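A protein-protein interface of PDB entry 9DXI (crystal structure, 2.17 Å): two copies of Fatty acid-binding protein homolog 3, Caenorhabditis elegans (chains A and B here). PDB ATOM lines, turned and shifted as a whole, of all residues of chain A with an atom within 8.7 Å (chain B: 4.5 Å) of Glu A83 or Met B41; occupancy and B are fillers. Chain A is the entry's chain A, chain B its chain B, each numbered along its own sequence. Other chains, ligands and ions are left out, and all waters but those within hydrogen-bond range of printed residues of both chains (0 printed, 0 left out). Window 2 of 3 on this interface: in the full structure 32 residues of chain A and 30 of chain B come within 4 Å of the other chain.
The side-chain carboxylate of Glu A83 lies close to the side-chain sulfur of Met B41, 3.5 Å away.
O of Ala A91 lies within hydrogen-bond range of N of Leu A110 (3.1 Å).
CB of Ala B45 touches OE1 of Glu A85, at 3.5 Å.
CB of Ala A91 touches CG1 of Val B38 (3.5 Å).
Glu A83 touches one residue of chain B.
Printed residues of chain B within 4 Å of Glu A85: Ala B45 (3.5 Å).
Of the printed residues of chain B, Ala A91 touches Val B38 (3.5 Å).
Of the printed residues of chain A, Val B38 touches Ala A91.
Met B41 touches just one residue of chain A: Glu A83.
The nearest printed residue of chain A that does not touch Val B38 is Leu A110 (4.02 Å).
Hydrophobic or aromatic side chains of chain A that line the printed part of chain B: Ala A91.
Hydrophobic or aromatic side chains of chain B that line the printed part of chain A: Val B38, Met B41 and Ala B45.
Among the printed residues, no Asp or Glu carboxylate lies within 4 Å of a Lys or Arg side-chain nitrogen of the other chain.
No position is printed for both chains.
Of the 3 pairs that touch across the chains among the printed residues, none has its exchanged pair printed and touching as well.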
ATOM      1  N   TYR A  73     -21.770  -8.845   1.024  1.00  0.00           N
ATOM      2  CA  TYR A  73     -20.797  -9.702   1.691  1.00  0.00           C
ATOM      3  C   TYR A  73     -21.202 -11.148   1.439  1.00  0.00           C
ATOM      4  O   TYR A  73     -22.287 -11.566   1.847  1.00  0.00           O
ATOM      5  CB  TYR A  73     -20.729  -9.409   3.191  1.00  0.00           C
ATOM      6  CG  TYR A  73     -20.357  -7.985   3.521  1.00  0.00           C
ATOM      7  CD1 TYR A  73     -19.053  -7.542   3.379  1.00  0.00           C
ATOM      8  CD2 TYR A  73     -21.309  -7.086   3.990  1.00  0.00           C
ATOM      9  CE1 TYR A  73     -18.704  -6.241   3.681  1.00  0.00           C
ATOM     10  CE2 TYR A  73     -20.969  -5.778   4.298  1.00  0.00           C
ATOM     11  CZ  TYR A  73     -19.663  -5.363   4.141  1.00  0.00           C
ATOM     12  OH  TYR A  73     -19.310  -4.067   4.441  1.00  0.00           O
ATOM     13  N   TRP A  76     -19.308 -15.819   3.717  1.00  0.00           N
ATOM     14  CA  TRP A  76     -18.729 -15.712   5.048  1.00  0.00           C
ATOM     15  C   TRP A  76     -19.268 -16.809   5.961  1.00  0.00           C
ATOM     16  O   TRP A  76     -20.310 -17.418   5.703  1.00  0.00           O
ATOM     17  CB  TRP A  76     -18.985 -14.331   5.666  1.00  0.00           C
ATOM     18  CG  TRP A  76     -20.400 -13.819   5.588  1.00  0.00           C
ATOM     19  CD1 TRP A  76     -20.909 -12.965   4.652  1.00  0.00           C
ATOM     20  CD2 TRP A  76     -21.472 -14.093   6.502  1.00  0.00           C
ATOM     21  NE1 TRP A  76     -22.232 -12.705   4.915  1.00  0.00           N
ATOM     22  CE2 TRP A  76     -22.602 -13.383   6.046  1.00  0.00           C
ATOM     23  CE3 TRP A  76     -21.590 -14.876   7.654  1.00  0.00           C
ATOM     24  CZ2 TRP A  76     -23.830 -13.432   6.701  1.00  0.00           C
ATOM     25  CZ3 TRP A  76     -22.813 -14.924   8.301  1.00  0.00           C
ATOM     26  CH2 TRP A  76     -23.914 -14.205   7.826  1.00  0.00           C
ATOM     27  N   LYS A  80     -15.894 -16.407  11.903  1.00  0.00           N
ATOM     28  CA  LYS A  80     -14.639 -16.305  11.123  1.00  0.00           C
ATOM     29  C   LYS A  80     -14.473 -14.891  10.567  1.00  0.00           C
ATOM     30  O   LYS A  80     -15.210 -14.512   9.656  1.00  0.00           O
ATOM     31  CB  LYS A  80     -14.598 -17.391  10.045  1.00  0.00           C
ATOM     32  CG  LYS A  80     -13.202 -17.758   9.568  1.00  0.00           C
ATOM     33  CD  LYS A  80     -13.158 -18.945   8.615  1.00  0.00           C
ATOM     34  CE  LYS A  80     -12.008 -19.859   8.899  1.00  0.00           C
ATOM     35  NZ  LYS A  80     -11.784 -20.822   7.820  1.00  0.00           N
ATOM     36  N   THR A  81     -13.496 -14.171  11.092  1.00  0.00           N
ATOM     37  CA  THR A  81     -13.248 -12.790  10.672  1.00  0.00           C
ATOM     38  C   THR A  81     -12.726 -12.776   9.268  1.00  0.00           C
ATOM     39  O   THR A  81     -11.968 -13.685   8.912  1.00  0.00           O
ATOM     40  CB  THR A  81     -12.252 -12.174  11.643  1.00  0.00           C
ATOM     41  OG1 THR A  81     -12.801 -12.378  12.938  1.00  0.00           O
ATOM     42  CG2 THR A  81     -12.054 -10.691  11.401  1.00  0.00           C
ATOM     43  N   PHE A  82     -13.123 -11.773   8.499  1.00  0.00           N
ATOM     44  CA  PHE A  82     -12.661 -11.645   7.098  1.00  0.00           C
ATOM     45  C   PHE A  82     -12.246 -10.218   6.872  1.00  0.00           C
ATOM     46  O   PHE A  82     -12.596  -9.325   7.654  1.00  0.00           O
ATOM     47  CB  PHE A  82     -13.698 -12.112   6.073  1.00  0.00           C
ATOM     48  CG  PHE A  82     -15.027 -11.377   5.986  1.00  0.00           C
ATOM     49  CD1 PHE A  82     -15.172 -10.261   5.173  1.00  0.00           C
ATOM     50  CD2 PHE A  82     -16.139 -11.837   6.676  1.00  0.00           C
ATOM     51  CE1 PHE A  82     -16.390  -9.609   5.080  1.00  0.00           C
ATOM     52  CE2 PHE A  82     -17.352 -11.179   6.580  1.00  0.00           C
ATOM     53  CZ  PHE A  82     -17.475 -10.070   5.782  1.00  0.00           C
ATOM     54  N   GLU A  83     -11.475 -10.015   5.818  1.00  0.00           N
ATOM     55  CA  GLU A  83     -10.958  -8.666   5.525  1.00  0.00           C
ATOM     56  C   GLU A  83     -11.584  -8.199   4.218  1.00  0.00           C
ATOM     57  O   GLU A  83     -11.656  -9.005   3.280  1.00  0.00           O
ATOM     58  CB  GLU A  83      -9.441  -8.743   5.407  1.00  0.00           C
ATOM     59  CG  GLU A  83      -8.754  -9.080   6.728  1.00  0.00           C
ATOM     60  CD  GLU A  83      -7.242  -9.245   6.681  1.00  0.00           C
ATOM     61  OE1 GLU A  83      -6.679  -9.289   5.567  1.00  0.00           O
ATOM     62  OE2 GLU A  83      -6.625  -9.339   7.762  1.00  0.00           O
ATOM     63  N   ALA A  84     -12.000  -6.938   4.166  1.00  0.00           N
ATOM     64  CA  ALA A  84     -12.611  -6.387   2.940  1.00  0.00           C
ATOM     65  C   ALA A  84     -11.833  -5.161   2.486  1.00  0.00           C
ATOM     66  O   ALA A  84     -11.497  -4.315   3.337  1.00  0.00           O
ATOM     67  CB  ALA A  84     -14.051  -6.055   3.195  1.00  0.00           C
ATOM     68  N   GLU A  85     -11.586  -5.058   1.180  1.00  0.00           N
ATOM     69  CA  GLU A  85     -10.741  -3.959   0.660  1.00  0.00           C
ATOM     70  C   GLU A  85     -11.525  -3.103  -0.332  1.00  0.00           C
ATOM     71  O   GLU A  85     -11.994  -3.664  -1.342  1.00  0.00           O
ATOM     72  CB  GLU A  85      -9.550  -4.568  -0.070  1.00  0.00           C
ATOM     73  CG  GLU A  85      -8.575  -5.284   0.860  1.00  0.00           C
ATOM     74  CD  GLU A  85      -8.896  -6.751   1.072  1.00  0.00           C
ATOM     75  OE1 GLU A  85      -9.697  -7.293   0.283  1.00  0.00           O
ATOM     76  OE2 GLU A  85      -8.349  -7.349   2.024  1.00  0.00           O
ATOM     77  N   GLY A  86     -11.642  -1.800  -0.062  1.00  0.00           N
ATOM     78  CA  GLY A  86     -12.373  -0.888  -0.963  1.00  0.00           C
ATOM     79  C   GLY A  86     -11.422  -0.069  -1.816  1.00  0.00           C
ATOM     80  O   GLY A  86     -10.219  -0.029  -1.483  1.00  0.00           O
ATOM     81  N   VAL A  90      -9.476   1.393   2.707  1.00  0.00           N
ATOM     82  CA  VAL A  90      -9.749   1.365   4.176  1.00  0.00           C
ATOM     83  C   VAL A  90     -10.074  -0.088   4.562  1.00  0.00           C
ATOM     84  O   VAL A  90     -11.248  -0.486   4.413  1.00  0.00           O
ATOM     85  CB  VAL A  90     -10.895   2.314   4.574  1.00  0.00           C
ATOM     86  CG1 VAL A  90     -10.386   3.520   5.354  1.00  0.00           C
ATOM     87  CG2 VAL A  90     -11.711   2.756   3.366  1.00  0.00           C
ATOM     88  N   ALA A  91      -9.076  -0.849   5.019  1.00  0.00           N
ATOM     89  CA  ALA A  91      -9.292  -2.278   5.354  1.00  0.00           C
ATOM     90  C   ALA A  91     -10.503  -2.424   6.280  1.00  0.00           C
ATOM     91  O   ALA A  91     -10.581  -1.695   7.293  1.00  0.00           O
ATOM     92  CB  ALA A  91      -8.046  -2.856   5.982  1.00  0.00           C
ATOM     93  N   HIS A  92     -11.411  -3.347   5.947  1.00  0.00           N
ATOM     94  CA  HIS A  92     -12.632  -3.558   6.772  1.00  0.00           C
ATOM     95  C   HIS A  92     -12.586  -4.947   7.417  1.00  0.00           C
ATOM     96  O   HIS A  92     -12.797  -5.953   6.706  1.00  0.00           O
ATOM     97  CB  HIS A  92     -13.894  -3.391   5.919  1.00  0.00           C
ATOM     98  CG  HIS A  92     -14.002  -2.066   5.245  1.00  0.00           C
ATOM     99  ND1 HIS A  92     -14.037  -0.877   5.940  1.00  0.00           N
ATOM    100  CD2 HIS A  92     -14.087  -1.741   3.948  1.00  0.00           C
ATOM    101  CE1 HIS A  92     -14.141   0.128   5.081  1.00  0.00           C
ATOM    102  NE2 HIS A  92     -14.170  -0.375   3.866  1.00  0.00           N
ATOM    103  N   LYS A  93     -12.318  -5.002   8.725  1.00  0.00           N
ATOM    104  CA  LYS A  93     -12.316  -6.301   9.449  1.00  0.00           C
ATOM    105  C   LYS A  93     -13.756  -6.619   9.882  1.00  0.00           C
ATOM    106  O   LYS A  93     -14.157  -6.163  10.975  1.00  0.00           O
ATOM    107  CB  LYS A  93     -11.380  -6.246  10.660  1.00  0.00           C
ATOM    108  CG  LYS A  93     -11.257  -7.555  11.425  1.00  0.00           C
ATOM    109  CD  LYS A  93     -10.280  -7.469  12.591  1.00  0.00           C
ATOM    110  CE  LYS A  93     -10.187  -8.755  13.347  1.00  0.00           C
ATOM    111  NZ  LYS A  93      -9.244  -8.657  14.465  1.00  0.00           N
ATOM    112  N   ILE A  94     -14.497  -7.366   9.057  1.00  0.00           N
ATOM    113  CA  ILE A  94     -15.929  -7.654   9.369  1.00  0.00           C
ATOM    114  C   ILE A  94     -16.054  -9.084   9.916  1.00  0.00           C
ATOM    115  O   ILE A  94     -15.413  -9.994   9.344  1.00  0.00           O
ATOM    116  CB  ILE A  94     -16.814  -7.437   8.128  1.00  0.00           C
ATOM    117  CG1 ILE A  94     -16.549  -6.077   7.490  1.00  0.00           C
ATOM    118  CG2 ILE A  94     -18.293  -7.625   8.467  1.00  0.00           C
ATOM    119  CD1 ILE A  94     -16.198  -6.144   6.018  1.00  0.00           C
ATOM    120  N   THR A  95     -16.841  -9.265  10.982  1.00  0.00           N
ATOM    121  CA  THR A  95     -17.047 -10.606  11.570  1.00  0.00           C
ATOM    122  C   THR A  95     -18.529 -10.831  11.775  1.00  0.00           C
ATOM    123  O   THR A  95     -19.211  -9.887  12.227  1.00  0.00           O
ATOM    124  CB  THR A  95     -16.285 -10.719  12.890  1.00  0.00           C
ATOM    125  OG1 THR A  95     -15.009 -10.132  12.658  1.00  0.00           O
ATOM    126  CG2 THR A  95     -16.122 -12.160  13.340  1.00  0.00           C
ATOM    127  N   ILE A 108     -14.543  -3.401  11.818  1.00  0.00           N
ATOM    128  CA  ILE A 108     -13.367  -2.674  12.378  1.00  0.00           C
ATOM    129  C   ILE A 108     -12.569  -2.112  11.200  1.00  0.00           C
ATOM    130  O   ILE A 108     -12.263  -2.886  10.282  1.00  0.00           O
ATOM    131  CB  ILE A 108     -12.484  -3.574  13.258  1.00  0.00           C
ATOM    132  CG1 ILE A 108     -13.161  -3.951  14.570  1.00  0.00           C
ATOM    133  CG2 ILE A 108     -11.127  -2.917  13.503  1.00  0.00           C
ATOM    134  CD1 ILE A 108     -12.420  -5.016  15.354  1.00  0.00           C
ATOM    135  N   LEU A 110      -9.058  -0.935   9.916  1.00  0.00           N
ATOM    136  CA  LEU A 110      -7.674  -1.149  10.401  1.00  0.00           C
ATOM    137  C   LEU A 110      -6.786   0.041   9.998  1.00  0.00           C
ATOM    138  O   LEU A 110      -7.063   1.159  10.485  1.00  0.00           O
ATOM    139  CB  LEU A 110      -7.203  -2.473   9.808  1.00  0.00           C
ATOM    140  CG  LEU A 110      -8.168  -3.652   9.961  1.00  0.00           C
ATOM    141  CD1 LEU A 110      -7.757  -4.799   9.057  1.00  0.00           C
ATOM    142  CD2 LEU A 110      -8.195  -4.105  11.405  1.00  0.00           C
ATOM    143  N   PHE B  37       1.593  -3.560   8.049  1.00  0.00           N
ATOM    144  CA  PHE B  37       0.875  -4.833   8.060  1.00  0.00           C
ATOM    145  C   PHE B  37      -0.347  -4.776   7.153  1.00  0.00           C
ATOM    146  O   PHE B  37      -0.619  -5.714   6.394  1.00  0.00           O
ATOM    147  CB  PHE B  37       0.461  -5.203   9.487  1.00  0.00           C
ATOM    148  CG  PHE B  37       1.597  -5.669  10.354  1.00  0.00           C
ATOM    149  CD1 PHE B  37       2.570  -6.518   9.853  1.00  0.00           C
ATOM    150  CD2 PHE B  37       1.685  -5.260  11.676  1.00  0.00           C
ATOM    151  CE1 PHE B  37       3.615  -6.948  10.653  1.00  0.00           C
ATOM    152  CE2 PHE B  37       2.729  -5.677  12.476  1.00  0.00           C
ATOM    153  CZ  PHE B  37       3.697  -6.524  11.963  1.00  0.00           C
ATOM    154  N   VAL B  38      -1.100  -3.677   7.218  1.00  0.00           N
ATOM    155  CA  VAL B  38      -2.310  -3.566   6.413  1.00  0.00           C
ATOM    156  C   VAL B  38      -1.965  -3.285   4.952  1.00  0.00           C
ATOM    157  O   VAL B  38      -2.648  -3.772   4.043  1.00  0.00           O
ATOM    158  CB  VAL B  38      -3.241  -2.488   7.001  1.00  0.00           C
ATOM    159  CG1 VAL B  38      -4.586  -2.521   6.310  1.00  0.00           C
ATOM    160  CG2 VAL B  38      -3.406  -2.686   8.499  1.00  0.00           C
ATOM    161  N   ARG B  39      -0.907  -2.512   4.694  1.00  0.00           N
ATOM    162  CA  ARG B  39      -0.466  -2.333   3.312  1.00  0.00           C
ATOM    163  C   ARG B  39      -0.143  -3.673   2.664  1.00  0.00           C
ATOM    164  O   ARG B  39      -0.435  -3.882   1.481  1.00  0.00           O
ATOM    165  CB  ARG B  39       0.747  -1.406   3.243  1.00  0.00           C
ATOM    166  CG  ARG B  39       0.469   0.026   3.674  1.00  0.00           C
ATOM    167  CD  ARG B  39       1.470   0.996   3.081  1.00  0.00           C
ATOM    168  NE  ARG B  39       2.854   0.583   3.277  1.00  0.00           N
ATOM    169  CZ  ARG B  39       3.599   0.924   4.320  1.00  0.00           C
ATOM    170  NH1 ARG B  39       3.111   1.647   5.313  1.00  0.00           N
ATOM    171  NH2 ARG B  39       4.867   0.527   4.366  1.00  0.00           N
ATOM    172  N   GLN B  40       0.433  -4.606   3.429  1.00  0.00           N
ATOM    173  CA  GLN B  40       0.811  -5.897   2.858  1.00  0.00           C
ATOM    174  C   GLN B  40      -0.409  -6.700   2.425  1.00  0.00           C
ATOM    175  O   GLN B  40      -0.378  -7.378   1.392  1.00  0.00           O
ATOM    176  CB  GLN B  40       1.645  -6.699   3.859  1.00  0.00           C
ATOM    177  CG  GLN B  40       3.051  -6.162   4.055  1.00  0.00           C
ATOM    178  CD  GLN B  40       3.818  -6.052   2.752  1.00  0.00           C
ATOM    179  OE1 GLN B  40       3.873  -4.987   2.139  1.00  0.00           O
ATOM    180  NE2 GLN B  40       4.415  -7.156   2.321  1.00  0.00           N
ATOM    181  N   MET B  41      -1.484  -6.619   3.208  1.00  0.00           N
ATOM    182  CA  MET B  41      -2.687  -7.423   2.879  1.00  0.00           C
ATOM    183  C   MET B  41      -3.444  -6.750   1.720  1.00  0.00           C
ATOM    184  O   MET B  41      -3.988  -7.471   0.868  1.00  0.00           O
ATOM    185  CB  MET B  41      -3.603  -7.644   4.090  1.00  0.00           C
ATOM    186  CG  MET B  41      -3.805  -6.460   5.003  1.00  0.00           C
ATOM    187  SD  MET B  41      -4.257  -6.937   6.684  1.00  0.00           S
ATOM    188  CE  MET B  41      -3.246  -8.411   6.865  1.00  0.00           C
ATOM    189  N   ILE B  42      -3.452  -5.423   1.687  1.00  0.00           N
ATOM    190  CA  ILE B  42      -4.179  -4.736   0.623  1.00  0.00           C
ATOM    191  C   ILE B  42      -3.531  -5.010  -0.728  1.00  0.00           C
ATOM    192  O   ILE B  42      -4.218  -5.306  -1.711  1.00  0.00           O
ATOM    193  CB  ILE B  42      -4.261  -3.227   0.912  1.00  0.00           C
ATOM    194  CG1 ILE B  42      -5.143  -2.959   2.128  1.00  0.00           C
ATOM    195  CG2 ILE B  42      -4.786  -2.472  -0.308  1.00  0.00           C
ATOM    196  CD1 ILE B  42      -5.018  -1.554   2.653  1.00  0.00           C
ATOM    197  N   LYS B  43      -2.199  -4.932  -0.796  1.00  0.00           N
ATOM    198  CA  LYS B  43      -1.495  -5.147  -2.056  1.00  0.00           C
ATOM    199  C   LYS B  43      -1.635  -6.575  -2.562  1.00  0.00           C
ATOM    200  O   LYS B  43      -1.406  -6.823  -3.751  1.00  0.00           O
ATOM    201  CB  LYS B  43      -0.021  -4.775  -1.885  1.00  0.00           C
ATOM    202  CG  LYS B  43       0.184  -3.284  -1.610  1.00  0.00           C
ATOM    203  CD  LYS B  43       1.436  -2.997  -0.782  1.00  0.00           C
ATOM    204  CE  LYS B  43       2.721  -3.368  -1.512  1.00  0.00           C
ATOM    205  NZ  LYS B  43       3.046  -4.820  -1.417  1.00  0.00           N
ATOM    206  N   LEU B  44      -2.022  -7.510  -1.697  1.00  0.00           N
ATOM    207  CA  LEU B  44      -2.219  -8.898  -2.091  1.00  0.00           C
ATOM    208  C   LEU B  44      -3.643  -9.191  -2.545  1.00  0.00           C
ATOM    209  O   LEU B  44      -3.858 -10.164  -3.278  1.00  0.00           O
ATOM    210  CB  LEU B  44      -1.857  -9.825  -0.924  1.00  0.00           C
ATOM    211  CG  LEU B  44      -1.216 -11.172  -1.253  1.00  0.00           C
ATOM    212  CD1 LEU B  44       0.053 -10.971  -2.067  1.00  0.00           C
ATOM    213  CD2 LEU B  44      -0.919 -11.937   0.029  1.00  0.00           C
ATOM    214  N   ALA B  45      -4.610  -8.372  -2.136  1.00  0.00           N
ATOM    215  CA  ALA B  45      -6.006  -8.619  -2.468  1.00  0.00           C
ATOM    216  C   ALA B  45      -6.239  -8.542  -3.972  1.00  0.00           C
ATOM    217  O   ALA B  45      -5.738  -7.643  -4.652  1.00  0.00           O
ATOM    218  CB  ALA B  45      -6.899  -7.610  -1.747  1.00  0.00           C
